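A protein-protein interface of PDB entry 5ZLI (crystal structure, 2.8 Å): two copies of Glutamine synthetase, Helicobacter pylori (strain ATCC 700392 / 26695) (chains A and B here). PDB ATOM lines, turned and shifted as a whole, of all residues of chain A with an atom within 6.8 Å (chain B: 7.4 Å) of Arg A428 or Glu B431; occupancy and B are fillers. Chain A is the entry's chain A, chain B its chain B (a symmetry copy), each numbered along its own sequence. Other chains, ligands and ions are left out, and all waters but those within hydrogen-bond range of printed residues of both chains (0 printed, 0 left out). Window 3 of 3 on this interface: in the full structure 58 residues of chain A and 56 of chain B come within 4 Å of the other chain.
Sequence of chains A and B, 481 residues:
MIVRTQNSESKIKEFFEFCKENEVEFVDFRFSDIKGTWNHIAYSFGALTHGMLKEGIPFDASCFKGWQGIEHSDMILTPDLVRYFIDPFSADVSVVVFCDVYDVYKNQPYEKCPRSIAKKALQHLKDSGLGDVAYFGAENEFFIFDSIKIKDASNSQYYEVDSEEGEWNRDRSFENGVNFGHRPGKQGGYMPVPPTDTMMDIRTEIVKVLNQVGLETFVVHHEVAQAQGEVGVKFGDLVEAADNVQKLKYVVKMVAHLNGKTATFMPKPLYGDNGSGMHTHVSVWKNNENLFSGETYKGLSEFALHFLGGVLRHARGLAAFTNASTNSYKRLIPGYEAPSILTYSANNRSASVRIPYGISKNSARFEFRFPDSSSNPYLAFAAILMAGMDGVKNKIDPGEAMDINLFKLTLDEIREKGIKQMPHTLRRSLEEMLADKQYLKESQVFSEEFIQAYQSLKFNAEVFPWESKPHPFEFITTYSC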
ATOM      1  N   ARG A 316      20.856  -0.025  13.098  1.00  0.00           N
ATOM      2  CA  ARG A 316      21.747  -1.162  12.828  1.00  0.00           C
ATOM      3  C   ARG A 316      23.018  -1.076  13.674  1.00  0.00           C
ATOM      4  O   ARG A 316      23.540  -2.098  14.121  1.00  0.00           O
ATOM      5  CB  ARG A 316      22.141  -1.255  11.343  1.00  0.00           C
ATOM      6  CG  ARG A 316      21.043  -1.477  10.340  1.00  0.00           C
ATOM      7  CD  ARG A 316      21.005  -2.909   9.870  1.00  0.00           C
ATOM      8  NE  ARG A 316      22.269  -3.390   9.301  1.00  0.00           N
ATOM      9  CZ  ARG A 316      22.508  -4.673   9.027  1.00  0.00           C
ATOM     10  NH1 ARG A 316      21.579  -5.584   9.283  1.00  0.00           N
ATOM     11  NH2 ARG A 316      23.665  -5.050   8.509  1.00  0.00           N
ATOM     12  N   GLY A 317      23.569   0.127  13.848  1.00  0.00           N
ATOM     13  CA  GLY A 317      24.678   0.299  14.771  1.00  0.00           C
ATOM     14  C   GLY A 317      24.256   0.474  16.217  1.00  0.00           C
ATOM     15  O   GLY A 317      24.972   0.042  17.125  1.00  0.00           O
ATOM     16  N   TYR A 329      20.678 -11.912  19.706  1.00  0.00           N
ATOM     17  CA  TYR A 329      20.278 -12.066  18.327  1.00  0.00           C
ATOM     18  C   TYR A 329      19.566 -13.371  18.091  1.00  0.00           C
ATOM     19  O   TYR A 329      18.845 -13.487  17.094  1.00  0.00           O
ATOM     20  CB  TYR A 329      21.500 -11.935  17.414  1.00  0.00           C
ATOM     21  CG  TYR A 329      22.135 -10.575  17.561  1.00  0.00           C
ATOM     22  CD1 TYR A 329      23.066 -10.330  18.576  1.00  0.00           C
ATOM     23  CD2 TYR A 329      21.745  -9.507  16.746  1.00  0.00           C
ATOM     24  CE1 TYR A 329      23.619  -9.070  18.750  1.00  0.00           C
ATOM     25  CE2 TYR A 329      22.299  -8.242  16.915  1.00  0.00           C
ATOM     26  CZ  TYR A 329      23.235  -8.044  17.919  1.00  0.00           C
ATOM     27  OH  TYR A 329      23.800  -6.839  18.139  1.00  0.00           O
ATOM     28  N   GLN A 421      16.789  -4.113   8.136  1.00  0.00           N
ATOM     29  CA  GLN A 421      16.395  -4.903   9.285  1.00  0.00           C
ATOM     30  C   GLN A 421      17.553  -5.051  10.259  1.00  0.00           C
ATOM     31  O   GLN A 421      18.712  -4.796   9.928  1.00  0.00           O
ATOM     32  CB  GLN A 421      15.870  -6.262   8.861  1.00  0.00           C
ATOM     33  CG  GLN A 421      16.858  -7.206   8.311  1.00  0.00           C
ATOM     34  CD  GLN A 421      16.146  -8.460   7.910  1.00  0.00           C
ATOM     35  OE1 GLN A 421      16.243  -9.491   8.579  1.00  0.00           O
ATOM     36  NE2 GLN A 421      15.378  -8.372   6.833  1.00  0.00           N
ATOM     37  N   MET A 422      17.229  -5.535  11.458  1.00  0.00           N
ATOM     38  CA  MET A 422      18.214  -5.630  12.518  1.00  0.00           C
ATOM     39  C   MET A 422      19.375  -6.527  12.093  1.00  0.00           C
ATOM     40  O   MET A 422      19.183  -7.508  11.363  1.00  0.00           O
ATOM     41  CB  MET A 422      17.569  -6.206  13.771  1.00  0.00           C
ATOM     42  CG  MET A 422      16.831  -5.203  14.601  1.00  0.00           C
ATOM     43  SD  MET A 422      18.048  -4.243  15.477  1.00  0.00           S
ATOM     44  CE  MET A 422      17.102  -2.886  16.142  1.00  0.00           C
ATOM     45  N   PRO A 423      20.590  -6.221  12.553  1.00  0.00           N
ATOM     46  CA  PRO A 423      21.726  -7.093  12.244  1.00  0.00           C
ATOM     47  C   PRO A 423      21.521  -8.449  12.880  1.00  0.00           C
ATOM     48  O   PRO A 423      20.941  -8.572  13.960  1.00  0.00           O
ATOM     49  CB  PRO A 423      22.924  -6.369  12.866  1.00  0.00           C
ATOM     50  CG  PRO A 423      22.356  -5.462  13.857  1.00  0.00           C
ATOM     51  CD  PRO A 423      20.970  -5.093  13.419  1.00  0.00           C
ATOM     52  N   HIS A 424      21.995  -9.472  12.195  1.00  0.00           N
ATOM     53  CA  HIS A 424      21.687 -10.816  12.628  1.00  0.00           C
ATOM     54  C   HIS A 424      22.676 -11.356  13.655  1.00  0.00           C
ATOM     55  O   HIS A 424      22.326 -12.282  14.392  1.00  0.00           O
ATOM     56  CB  HIS A 424      21.563 -11.714  11.397  1.00  0.00           C
ATOM     57  CG  HIS A 424      20.354 -11.403  10.568  1.00  0.00           C
ATOM     58  ND1 HIS A 424      20.431 -10.834   9.316  1.00  0.00           N
ATOM     59  CD2 HIS A 424      19.033 -11.560  10.827  1.00  0.00           C
ATOM     60  CE1 HIS A 424      19.211 -10.662   8.836  1.00  0.00           C
ATOM     61  NE2 HIS A 424      18.345 -11.095   9.731  1.00  0.00           N
ATOM     62  N   THR A 425      23.892 -10.814  13.725  1.00  0.00           N
ATOM     63  CA  THR A 425      24.846 -11.261  14.717  1.00  0.00           C
ATOM     64  C   THR A 425      25.372 -10.032  15.428  1.00  0.00           C
ATOM     65  O   THR A 425      25.286  -8.917  14.913  1.00  0.00           O
ATOM     66  CB  THR A 425      26.033 -12.054  14.108  1.00  0.00           C
ATOM     67  OG1 THR A 425      26.746 -11.239  13.171  1.00  0.00           O
ATOM     68  CG2 THR A 425      25.568 -13.342  13.415  1.00  0.00           C
ATOM     69  N   LEU A 426      25.973 -10.263  16.594  1.00  0.00           N
ATOM     70  CA  LEU A 426      26.622  -9.176  17.326  1.00  0.00           C
ATOM     71  C   LEU A 426      27.766  -8.567  16.543  1.00  0.00           C
ATOM     72  O   LEU A 426      28.087  -7.377  16.721  1.00  0.00           O
ATOM     73  CB  LEU A 426      27.177  -9.683  18.649  1.00  0.00           C
ATOM     74  CG  LEU A 426      27.790  -8.543  19.448  1.00  0.00           C
ATOM     75  CD1 LEU A 426      26.722  -7.491  19.666  1.00  0.00           C
ATOM     76  CD2 LEU A 426      28.372  -9.052  20.753  1.00  0.00           C
ATOM     77  N   ARG A 427      28.440  -9.374  15.727  1.00  0.00           N
ATOM     78  CA  ARG A 427      29.551  -8.831  14.974  1.00  0.00           C
ATOM     79  C   ARG A 427      29.079  -7.793  13.980  1.00  0.00           C
ATOM     80  O   ARG A 427      29.680  -6.722  13.878  1.00  0.00           O
ATOM     81  CB  ARG A 427      30.338  -9.929  14.279  1.00  0.00           C
ATOM     82  CG  ARG A 427      31.149  -9.327  13.194  1.00  0.00           C
ATOM     83  CD  ARG A 427      32.165 -10.246  12.739  1.00  0.00           C
ATOM     84  NE  ARG A 427      33.272 -10.088  13.655  1.00  0.00           N
ATOM     85  CZ  ARG A 427      34.173 -11.027  13.843  1.00  0.00           C
ATOM     86  NH1 ARG A 427      34.045 -12.137  13.147  1.00  0.00           N
ATOM     87  NH2 ARG A 427      35.178 -10.858  14.697  1.00  0.00           N
ATOM     88  N   ARG A 428      28.000  -8.079  13.235  1.00  0.00           N
ATOM     89  CA  ARG A 428      27.573  -7.080  12.267  1.00  0.00           C
ATOM     90  C   ARG A 428      27.138  -5.817  12.991  1.00  0.00           C
ATOM     91  O   ARG A 428      27.425  -4.710  12.526  1.00  0.00           O
ATOM     92  CB  ARG A 428      26.482  -7.626  11.326  1.00  0.00           C
ATOM     93  CG  ARG A 428      26.583  -7.045   9.854  1.00  0.00           C
ATOM     94  CD  ARG A 428      25.757  -7.812   8.766  1.00  0.00           C
ATOM     95  NE  ARG A 428      24.373  -8.023   9.200  1.00  0.00           N
ATOM     96  CZ  ARG A 428      23.432  -8.705   8.552  1.00  0.00           C
ATOM     97  NH1 ARG A 428      22.247  -8.795   9.101  1.00  0.00           N
ATOM     98  NH2 ARG A 428      23.659  -9.294   7.386  1.00  0.00           N
ATOM     99  N   SER A 429      26.551  -5.964  14.179  1.00  0.00           N
ATOM    100  CA  SER A 429      26.147  -4.805  14.972  1.00  0.00           C
ATOM    101  C   SER A 429      27.331  -3.927  15.347  1.00  0.00           C
ATOM    102  O   SER A 429      27.192  -2.704  15.481  1.00  0.00           O
ATOM    103  CB  SER A 429      25.444  -5.264  16.232  1.00  0.00           C
ATOM    104  OG  SER A 429      24.171  -4.698  16.282  1.00  0.00           O
ATOM    105  N   LEU A 430      28.480  -4.542  15.605  1.00  0.00           N
ATOM    106  CA  LEU A 430      29.667  -3.773  15.943  1.00  0.00           C
ATOM    107  C   LEU A 430      30.274  -3.115  14.709  1.00  0.00           C
ATOM    108  O   LEU A 430      30.648  -1.936  14.757  1.00  0.00           O
ATOM    109  CB  LEU A 430      30.693  -4.677  16.621  1.00  0.00           C
ATOM    110  CG  LEU A 430      30.315  -5.220  17.988  1.00  0.00           C
ATOM    111  CD1 LEU A 430      31.247  -6.367  18.323  1.00  0.00           C
ATOM    112  CD2 LEU A 430      30.450  -4.087  19.015  1.00  0.00           C
ATOM    113  N   GLU A 431      30.367  -3.853  13.597  1.00  0.00           N
ATOM    114  CA  GLU A 431      30.828  -3.260  12.346  1.00  0.00           C
ATOM    115  C   GLU A 431      30.052  -1.969  12.071  1.00  0.00           C
ATOM    116  O   GLU A 431      30.623  -0.870  12.031  1.00  0.00           O
ATOM    117  CB  GLU A 431      30.641  -4.270  11.184  1.00  0.00           C
ATOM    118  CG  GLU A 431      31.662  -5.470  11.093  1.00  0.00           C
ATOM    119  CD  GLU A 431      31.272  -6.606  10.071  1.00  0.00           C
ATOM    120  OE1 GLU A 431      31.954  -7.666  10.042  1.00  0.00           O
ATOM    121  OE2 GLU A 431      30.272  -6.466   9.321  1.00  0.00           O
ATOM    122  N   GLU A 432      28.722  -2.086  12.046  1.00  0.00           N
ATOM    123  CA  GLU A 432      27.868  -0.942  11.776  1.00  0.00           C
ATOM    124  C   GLU A 432      28.091   0.146  12.803  1.00  0.00           C
ATOM    125  O   GLU A 432      28.084   1.336  12.474  1.00  0.00           O
ATOM    126  CB  GLU A 432      26.396  -1.368  11.771  1.00  0.00           C
ATOM    127  CG  GLU A 432      26.019  -2.323  10.659  1.00  0.00           C
ATOM    128  CD  GLU A 432      25.476  -1.599   9.462  1.00  0.00           C
ATOM    129  OE1 GLU A 432      25.611  -2.132   8.337  1.00  0.00           O
ATOM    130  OE2 GLU A 432      24.949  -0.478   9.655  1.00  0.00           O
ATOM    131  N   MET A 433      28.299  -0.237  14.050  1.00  0.00           N
ATOM    132  CA  MET A 433      28.532   0.764  15.071  1.00  0.00           C
ATOM    133  C   MET A 433      29.801   1.550  14.763  1.00  0.00           C
ATOM    134  O   MET A 433      29.788   2.786  14.725  1.00  0.00           O
ATOM    135  CB  MET A 433      28.583   0.064  16.432  1.00  0.00           C
ATOM    136  CG  MET A 433      28.776   0.944  17.642  1.00  0.00           C
ATOM    137  SD  MET A 433      30.491   1.024  18.141  1.00  0.00           S
ATOM    138  CE  MET A 433      30.355   2.218  19.410  1.00  0.00           C
ATOM    139  N   PHE A 459      34.100  -7.982  21.539  1.00  0.00           N
ATOM    140  CA  PHE A 459      34.528  -9.031  20.615  1.00  0.00           C
ATOM    141  C   PHE A 459      35.091 -10.228  21.353  1.00  0.00           C
ATOM    142  O   PHE A 459      34.816 -11.374  20.970  1.00  0.00           O
ATOM    143  CB  PHE A 459      35.554  -8.534  19.593  1.00  0.00           C
ATOM    144  CG  PHE A 459      34.935  -8.070  18.305  1.00  0.00           C
ATOM    145  CD1 PHE A 459      34.387  -8.982  17.429  1.00  0.00           C
ATOM    146  CD2 PHE A 459      34.966  -6.753  17.935  1.00  0.00           C
ATOM    147  CE1 PHE A 459      33.812  -8.568  16.250  1.00  0.00           C
ATOM    148  CE2 PHE A 459      34.422  -6.349  16.747  1.00  0.00           C
ATOM    149  CZ  PHE A 459      33.844  -7.260  15.909  1.00  0.00           C
ATOM    150  N   ARG B 316      37.491 -15.426  -0.287  1.00  0.00           N
ATOM    151  CA  ARG B 316      36.422 -15.226   0.693  1.00  0.00           C
ATOM    152  C   ARG B 316      35.083 -15.758   0.193  1.00  0.00           C
ATOM    153  O   ARG B 316      34.272 -16.236   0.987  1.00  0.00           O
ATOM    154  CB  ARG B 316      36.322 -13.755   1.122  1.00  0.00           C
ATOM    155  CG  ARG B 316      37.611 -13.269   1.723  1.00  0.00           C
ATOM    156  CD  ARG B 316      37.407 -12.488   2.999  1.00  0.00           C
ATOM    157  NE  ARG B 316      36.160 -11.734   3.109  1.00  0.00           N
ATOM    158  CZ  ARG B 316      35.665 -11.305   4.274  1.00  0.00           C
ATOM    159  NH1 ARG B 316      36.311 -11.553   5.405  1.00  0.00           N
ATOM    160  NH2 ARG B 316      34.535 -10.623   4.317  1.00  0.00           N
ATOM    161  N   GLY B 317      34.805 -15.649  -1.107  1.00  0.00           N
ATOM    162  CA  GLY B 317      33.592 -16.257  -1.631  1.00  0.00           C
ATOM    163  C   GLY B 317      33.705 -17.751  -1.838  1.00  0.00           C
ATOM    164  O   GLY B 317      32.716 -18.473  -1.676  1.00  0.00           O
ATOM    165  N   ALA B 320      32.560 -20.474   0.876  1.00  0.00           N
ATOM    166  CA  ALA B 320      31.205 -21.028   0.854  1.00  0.00           C
ATOM    167  C   ALA B 320      31.122 -22.446   0.270  1.00  0.00           C
ATOM    168  O   ALA B 320      30.148 -23.161   0.538  1.00  0.00           O
ATOM    169  CB  ALA B 320      30.285 -20.077   0.095  1.00  0.00           C
ATOM    170  N   THR B 425      32.345 -16.083   9.392  1.00  0.00           N
ATOM    171  CA  THR B 425      31.166 -16.907   9.462  1.00  0.00           C
ATOM    172  C   THR B 425      30.810 -17.358   8.058  1.00  0.00           C
ATOM    173  O   THR B 425      31.209 -16.734   7.068  1.00  0.00           O
ATOM    174  CB  THR B 425      30.006 -16.128  10.120  1.00  0.00           C
ATOM    175  OG1 THR B 425      29.824 -14.866   9.459  1.00  0.00           O
ATOM    176  CG2 THR B 425      30.257 -15.893  11.573  1.00  0.00           C
ATOM    177  N   LEU B 426      30.027 -18.439   7.998  1.00  0.00           N
ATOM    178  CA  LEU B 426      29.458 -18.893   6.735  1.00  0.00           C
ATOM    179  C   LEU B 426      28.505 -17.862   6.135  1.00  0.00           C
ATOM    180  O   LEU B 426      28.357 -17.791   4.904  1.00  0.00           O
ATOM    181  CB  LEU B 426      28.727 -20.210   6.948  1.00  0.00           C
ATOM    182  CG  LEU B 426      27.982 -20.785   5.759  1.00  0.00           C
ATOM    183  CD1 LEU B 426      28.921 -20.975   4.605  1.00  0.00           C
ATOM    184  CD2 LEU B 426      27.353 -22.085   6.229  1.00  0.00           C
ATOM    185  N   ARG B 427      27.832 -17.074   6.979  1.00  0.00           N
ATOM    186  CA  ARG B 427      26.929 -16.060   6.457  1.00  0.00           C
ATOM    187  C   ARG B 427      27.704 -15.034   5.639  1.00  0.00           C
ATOM    188  O   ARG B 427      27.292 -14.674   4.529  1.00  0.00           O
ATOM    189  CB  ARG B 427      26.180 -15.369   7.594  1.00  0.00           C
ATOM    190  CG  ARG B 427      25.516 -14.054   7.175  1.00  0.00           C
ATOM    191  CD  ARG B 427      24.750 -13.472   8.315  1.00  0.00           C
ATOM    192  NE  ARG B 427      23.449 -14.089   8.430  1.00  0.00           N
ATOM    193  CZ  ARG B 427      22.367 -13.606   7.855  1.00  0.00           C
ATOM    194  NH1 ARG B 427      22.460 -12.502   7.135  1.00  0.00           N
ATOM    195  NH2 ARG B 427      21.207 -14.218   8.004  1.00  0.00           N
ATOM    196  N   ARG B 428      28.847 -14.560   6.162  1.00  0.00           N
ATOM    197  CA  ARG B 428      29.606 -13.599   5.382  1.00  0.00           C
ATOM    198  C   ARG B 428      30.186 -14.274   4.142  1.00  0.00           C
ATOM    199  O   ARG B 428      30.169 -13.671   3.067  1.00  0.00           O
ATOM    200  CB  ARG B 428      30.672 -12.919   6.255  1.00  0.00           C
ATOM    201  CG  ARG B 428      30.793 -11.394   5.995  1.00  0.00           C
ATOM    202  CD  ARG B 428      31.682 -10.683   7.006  1.00  0.00           C
ATOM    203  NE  ARG B 428      33.013 -11.287   7.138  1.00  0.00           N
ATOM    204  CZ  ARG B 428      33.897 -10.932   8.064  1.00  0.00           C
ATOM    205  NH1 ARG B 428      35.092 -11.508   8.134  1.00  0.00           N
ATOM    206  NH2 ARG B 428      33.560  -9.990   8.931  1.00  0.00           N
ATOM    207  N   SER B 429      30.601 -15.548   4.254  1.00  0.00           N
ATOM    208  CA  SER B 429      31.121 -16.288   3.107  1.00  0.00           C
ATOM    209  C   SER B 429      30.091 -16.422   1.998  1.00  0.00           C
ATOM    210  O   SER B 429      30.427 -16.301   0.816  1.00  0.00           O
ATOM    211  CB  SER B 429      31.551 -17.674   3.545  1.00  0.00           C
ATOM    212  OG  SER B 429      32.713 -17.580   4.314  1.00  0.00           O
ATOM    213  N   LEU B 430      28.823 -16.640   2.355  1.00  0.00           N
ATOM    214  CA  LEU B 430      27.814 -16.744   1.312  1.00  0.00           C
ATOM    215  C   LEU B 430      27.562 -15.384   0.694  1.00  0.00           C
ATOM    216  O   LEU B 430      27.471 -15.264  -0.535  1.00  0.00           O
ATOM    217  CB  LEU B 430      26.525 -17.342   1.860  1.00  0.00           C
ATOM    218  CG  LEU B 430      26.700 -18.817   2.219  1.00  0.00           C
ATOM    219  CD1 LEU B 430      25.532 -19.355   3.029  1.00  0.00           C
ATOM    220  CD2 LEU B 430      26.869 -19.622   0.948  1.00  0.00           C
ATOM    221  N   GLU B 431      27.472 -14.348   1.529  1.00  0.00           N
ATOM    222  CA  GLU B 431      27.426 -12.983   1.027  1.00  0.00           C
ATOM    223  C   GLU B 431      28.598 -12.709   0.066  1.00  0.00           C
ATOM    224  O   GLU B 431      28.401 -12.249  -1.062  1.00  0.00           O
ATOM    225  CB  GLU B 431      27.407 -12.040   2.233  1.00  0.00           C
ATOM    226  CG  GLU B 431      26.031 -12.011   2.917  1.00  0.00           C
ATOM    227  CD  GLU B 431      26.033 -11.402   4.327  1.00  0.00           C
ATOM    228  OE1 GLU B 431      27.092 -10.922   4.811  1.00  0.00           O
ATOM    229  OE2 GLU B 431      24.946 -11.410   4.949  1.00  0.00           O
ATOM    230  N   GLU B 432      29.824 -13.029   0.484  1.00  0.00           N
ATOM    231  CA  GLU B 432      30.972 -12.799  -0.388  1.00  0.00           C
ATOM    232  C   GLU B 432      30.844 -13.611  -1.666  1.00  0.00           C
ATOM    233  O   GLU B 432      31.238 -13.147  -2.742  1.00  0.00           O
ATOM    234  CB  GLU B 432      32.280 -13.131   0.333  1.00  0.00           C
ATOM    235  CG  GLU B 432      32.457 -12.269   1.566  1.00  0.00           C
ATOM    236  CD  GLU B 432      33.201 -10.992   1.329  1.00  0.00           C
ATOM    237  OE1 GLU B 432      34.025 -10.941   0.395  1.00  0.00           O
ATOM    238  OE2 GLU B 432      32.910 -10.015   2.059  1.00  0.00           O
ATOM    239  N   MET B 433      30.326 -14.833  -1.572  1.00  0.00           N
ATOM    240  CA  MET B 433      30.140 -15.606  -2.792  1.00  0.00           C
ATOM    241  C   MET B 433      29.073 -14.996  -3.676  1.00  0.00           C
ATOM    242  O   MET B 433      29.253 -14.866  -4.891  1.00  0.00           O
ATOM    243  CB  MET B 433      29.765 -17.041  -2.504  1.00  0.00           C
ATOM    244  CG  MET B 433      29.641 -17.788  -3.818  1.00  0.00           C
ATOM    245  SD  MET B 433      28.508 -19.172  -3.809  1.00  0.00           S
ATOM    246  CE  MET B 433      26.937 -18.336  -3.715  1.00  0.00           C
ATOM    247  N   LEU B 434      27.933 -14.653  -3.084  1.00  0.00           N
ATOM    248  CA  LEU B 434      26.820 -14.161  -3.878  1.00  0.00           C
ATOM    249  C   LEU B 434      27.152 -12.841  -4.542  1.00  0.00           C
ATOM    250  O   LEU B 434      26.603 -12.539  -5.602  1.00  0.00           O
ATOM    251  CB  LEU B 434      25.593 -14.008  -2.991  1.00  0.00           C
ATOM    252  CG  LEU B 434      24.965 -15.325  -2.583  1.00  0.00           C
ATOM    253  CD1 LEU B 434      23.837 -15.109  -1.569  1.00  0.00           C
ATOM    254  CD2 LEU B 434      24.434 -15.966  -3.834  1.00  0.00           C
ATOM    255  N   ALA B 435      28.059 -12.065  -3.966  1.00  0.00           N
ATOM    256  CA  ALA B 435      28.493 -10.806  -4.552  1.00  0.00           C
ATOM    257  C   ALA B 435      29.672 -10.977  -5.502  1.00  0.00           C
ATOM    258  O   ALA B 435      30.182  -9.987  -6.030  1.00  0.00           O
ATOM    259  CB  ALA B 435      28.845  -9.812  -3.459  1.00  0.00           C
ATOM    260  N   ASP B 436      30.110 -12.203  -5.734  1.00  0.00           N
ATOM    261  CA  ASP B 436      31.206 -12.537  -6.641  1.00  0.00           C
ATOM    262  C   ASP B 436      30.957 -13.957  -7.120  1.00  0.00           C
ATOM    263  O   ASP B 436      31.496 -14.933  -6.592  1.00  0.00           O
ATOM    264  CB  ASP B 436      32.579 -12.474  -5.987  1.00  0.00           C
ATOM    265  CG  ASP B 436      33.666 -12.506  -7.000  1.00  0.00           C
ATOM    266  OD1 ASP B 436      34.852 -12.579  -6.607  1.00  0.00           O
ATOM    267  OD2 ASP B 436      33.307 -12.581  -8.199  1.00  0.00           O
ATOM    268  N   GLN B 455      22.596 -21.452  -1.973  1.00  0.00           N
ATOM    269  CA  GLN B 455      22.468 -20.377  -0.999  1.00  0.00           C
ATOM    270  C   GLN B 455      21.288 -20.632  -0.073  1.00  0.00           C
ATOM    271  O   GLN B 455      21.404 -20.521   1.145  1.00  0.00           O
ATOM    272  CB  GLN B 455      22.324 -19.036  -1.726  1.00  0.00           C
ATOM    273  CG  GLN B 455      21.706 -17.914  -0.881  1.00  0.00           C
ATOM    274  CD  GLN B 455      20.203 -17.754  -1.111  1.00  0.00           C
ATOM    275  OE1 GLN B 455      19.642 -18.247  -2.106  1.00  0.00           O
ATOM    276  NE2 GLN B 455      19.540 -17.071  -0.173  1.00  0.00           N
ATOM    277  N   PHE B 459      21.735 -21.429   4.115  1.00  0.00           N
ATOM    278  CA  PHE B 459      21.105 -20.559   5.088  1.00  0.00           C
ATOM    279  C   PHE B 459      20.083 -21.330   5.931  1.00  0.00           C
ATOM    280  O   PHE B 459      20.113 -21.233   7.164  1.00  0.00           O
ATOM    281  CB  PHE B 459      20.480 -19.373   4.360  1.00  0.00           C
ATOM    282  CG  PHE B 459      21.419 -18.204   4.178  1.00  0.00           C
ATOM    283  CD1 PHE B 459      21.641 -17.301   5.195  1.00  0.00           C
ATOM    284  CD2 PHE B 459      22.096 -18.024   2.990  1.00  0.00           C
ATOM    285  CE1 PHE B 459      22.513 -16.228   5.014  1.00  0.00           C
ATOM    286  CE2 PHE B 459      22.958 -16.955   2.817  1.00  0.00           C
ATOM    287  CZ  PHE B 459      23.168 -16.069   3.819  1.00  0.00           C
ATOM    288  N   GLU B 467      22.311 -19.371  14.175  1.00  0.00           N
ATOM    289  CA  GLU B 467      22.022 -18.002  14.605  1.00  0.00           C
ATOM    290  C   GLU B 467      20.838 -17.913  15.566  1.00  0.00           C
ATOM    291  O   GLU B 467      20.676 -16.887  16.236  1.00  0.00           O
ATOM    292  CB  GLU B 467      21.740 -17.100  13.390  1.00  0.00           C
ATOM    293  CG  GLU B 467      22.921 -16.254  12.852  1.00  0.00           C
ATOM    294  CD  GLU B 467      22.602 -15.519  11.518  1.00  0.00           C
ATOM    295  OE1 GLU B 467      23.461 -14.727  11.051  1.00  0.00           O
ATOM    296  OE2 GLU B 467      21.498 -15.718  10.940  1.00  0.00           O
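The guanidinium group of Arg A428 is in salt-bridge range of the side-chain carboxylate of Glu B431, at 3.5 Å. NH1 of Arg B427 is in hydrogen-bond range of ND1 of His A424 (3.4 Å). The guanidinium group of Arg A428 lies close to the guanidinium group of Arg B427 (3.4 Å). NH2 of Arg B428 is in salt-bridge range of OE1 of Glu A431, 3.0 Å away.
The backbone NH (N) of Arg B428 is in hydrogen-bond range of the side-chain hydroxyl (OG1) of Thr B425, at 3.5 Å. NH1 of Arg B427 is in salt-bridge range of OE2 of Glu B431 (3.5 Å). The side-chain amide oxygen of Gln A421 is in hydrogen-bond range of a ring nitrogen (NE2) of His A424. OH of Tyr A329 lies within hydrogen-bond range of OG of Ser A429 (2.9 Å). The guanidinium group of Arg B427 is in salt-bridge range of the side-chain carboxylate of Glu B467, 2.7 Å away. OG1 of Thr A425 is in hydrogen-bond range of N of Arg A428, at 3.4 Å.
Among the printed residues, pairs that only touch across the chains: Thr A425 with Glu B467 (3.5 Å), His A424 with Glu B467 (3.6 Å) and Tyr A329 with Glu B467 (3.96 Å).
Of chain B, only Arg B427 and Glu B431 come within 4 Å of Arg A428. Of the printed residues of chain A, Glu B431 touches Arg A428 (3.5 Å). Of the printed residues of chain B, Tyr A329 touches Glu B467 (3.96 Å). Printed residues of chain B within 4 Å of His A424: Arg B427 (3.4 Å) and Glu B467 (3.6 Å). Leu A430 touches none of the printed residues of chain B. Arg B316 touches none of the printed residues of chain A. The nearest residue of chain A that does not touch Glu B431 is His A424 (6.3 Å). The nearest printed residue of chain B that does not touch Thr A425 is Arg B427 (5.2 Å).
Of the 17 printed residues of chain A, 5 touch a printed residue of chain B. Printed residues of chain A that touch a printed residue of chain B: Tyr A329, His A424, Thr A425, Arg A428 and Glu A431. Hydrophobic or aromatic side chains of chain A that line the printed part of chain B: His A424. Among the printed residues, 7 pairs touch across the chains. Among the printed residues, Asp or Glu carboxylates within 4 Å of a Lys or Arg side-chain nitrogen of the other chain: Arg A428 with Glu B431 (3.5 Å) and Glu A431 with Arg B428 (3.0 Å).
Arg A428 touches Arg B427, but with the chains exchanged Arg A427 does not touch Arg B428 (4.1 Å). Arg A428 touches Glu B431, and with the chains exchanged Glu A431 touches Arg B428. Of the 7 pairs that touch across the chains among the printed residues, 2 have their exchanged pair printed and touching as well.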
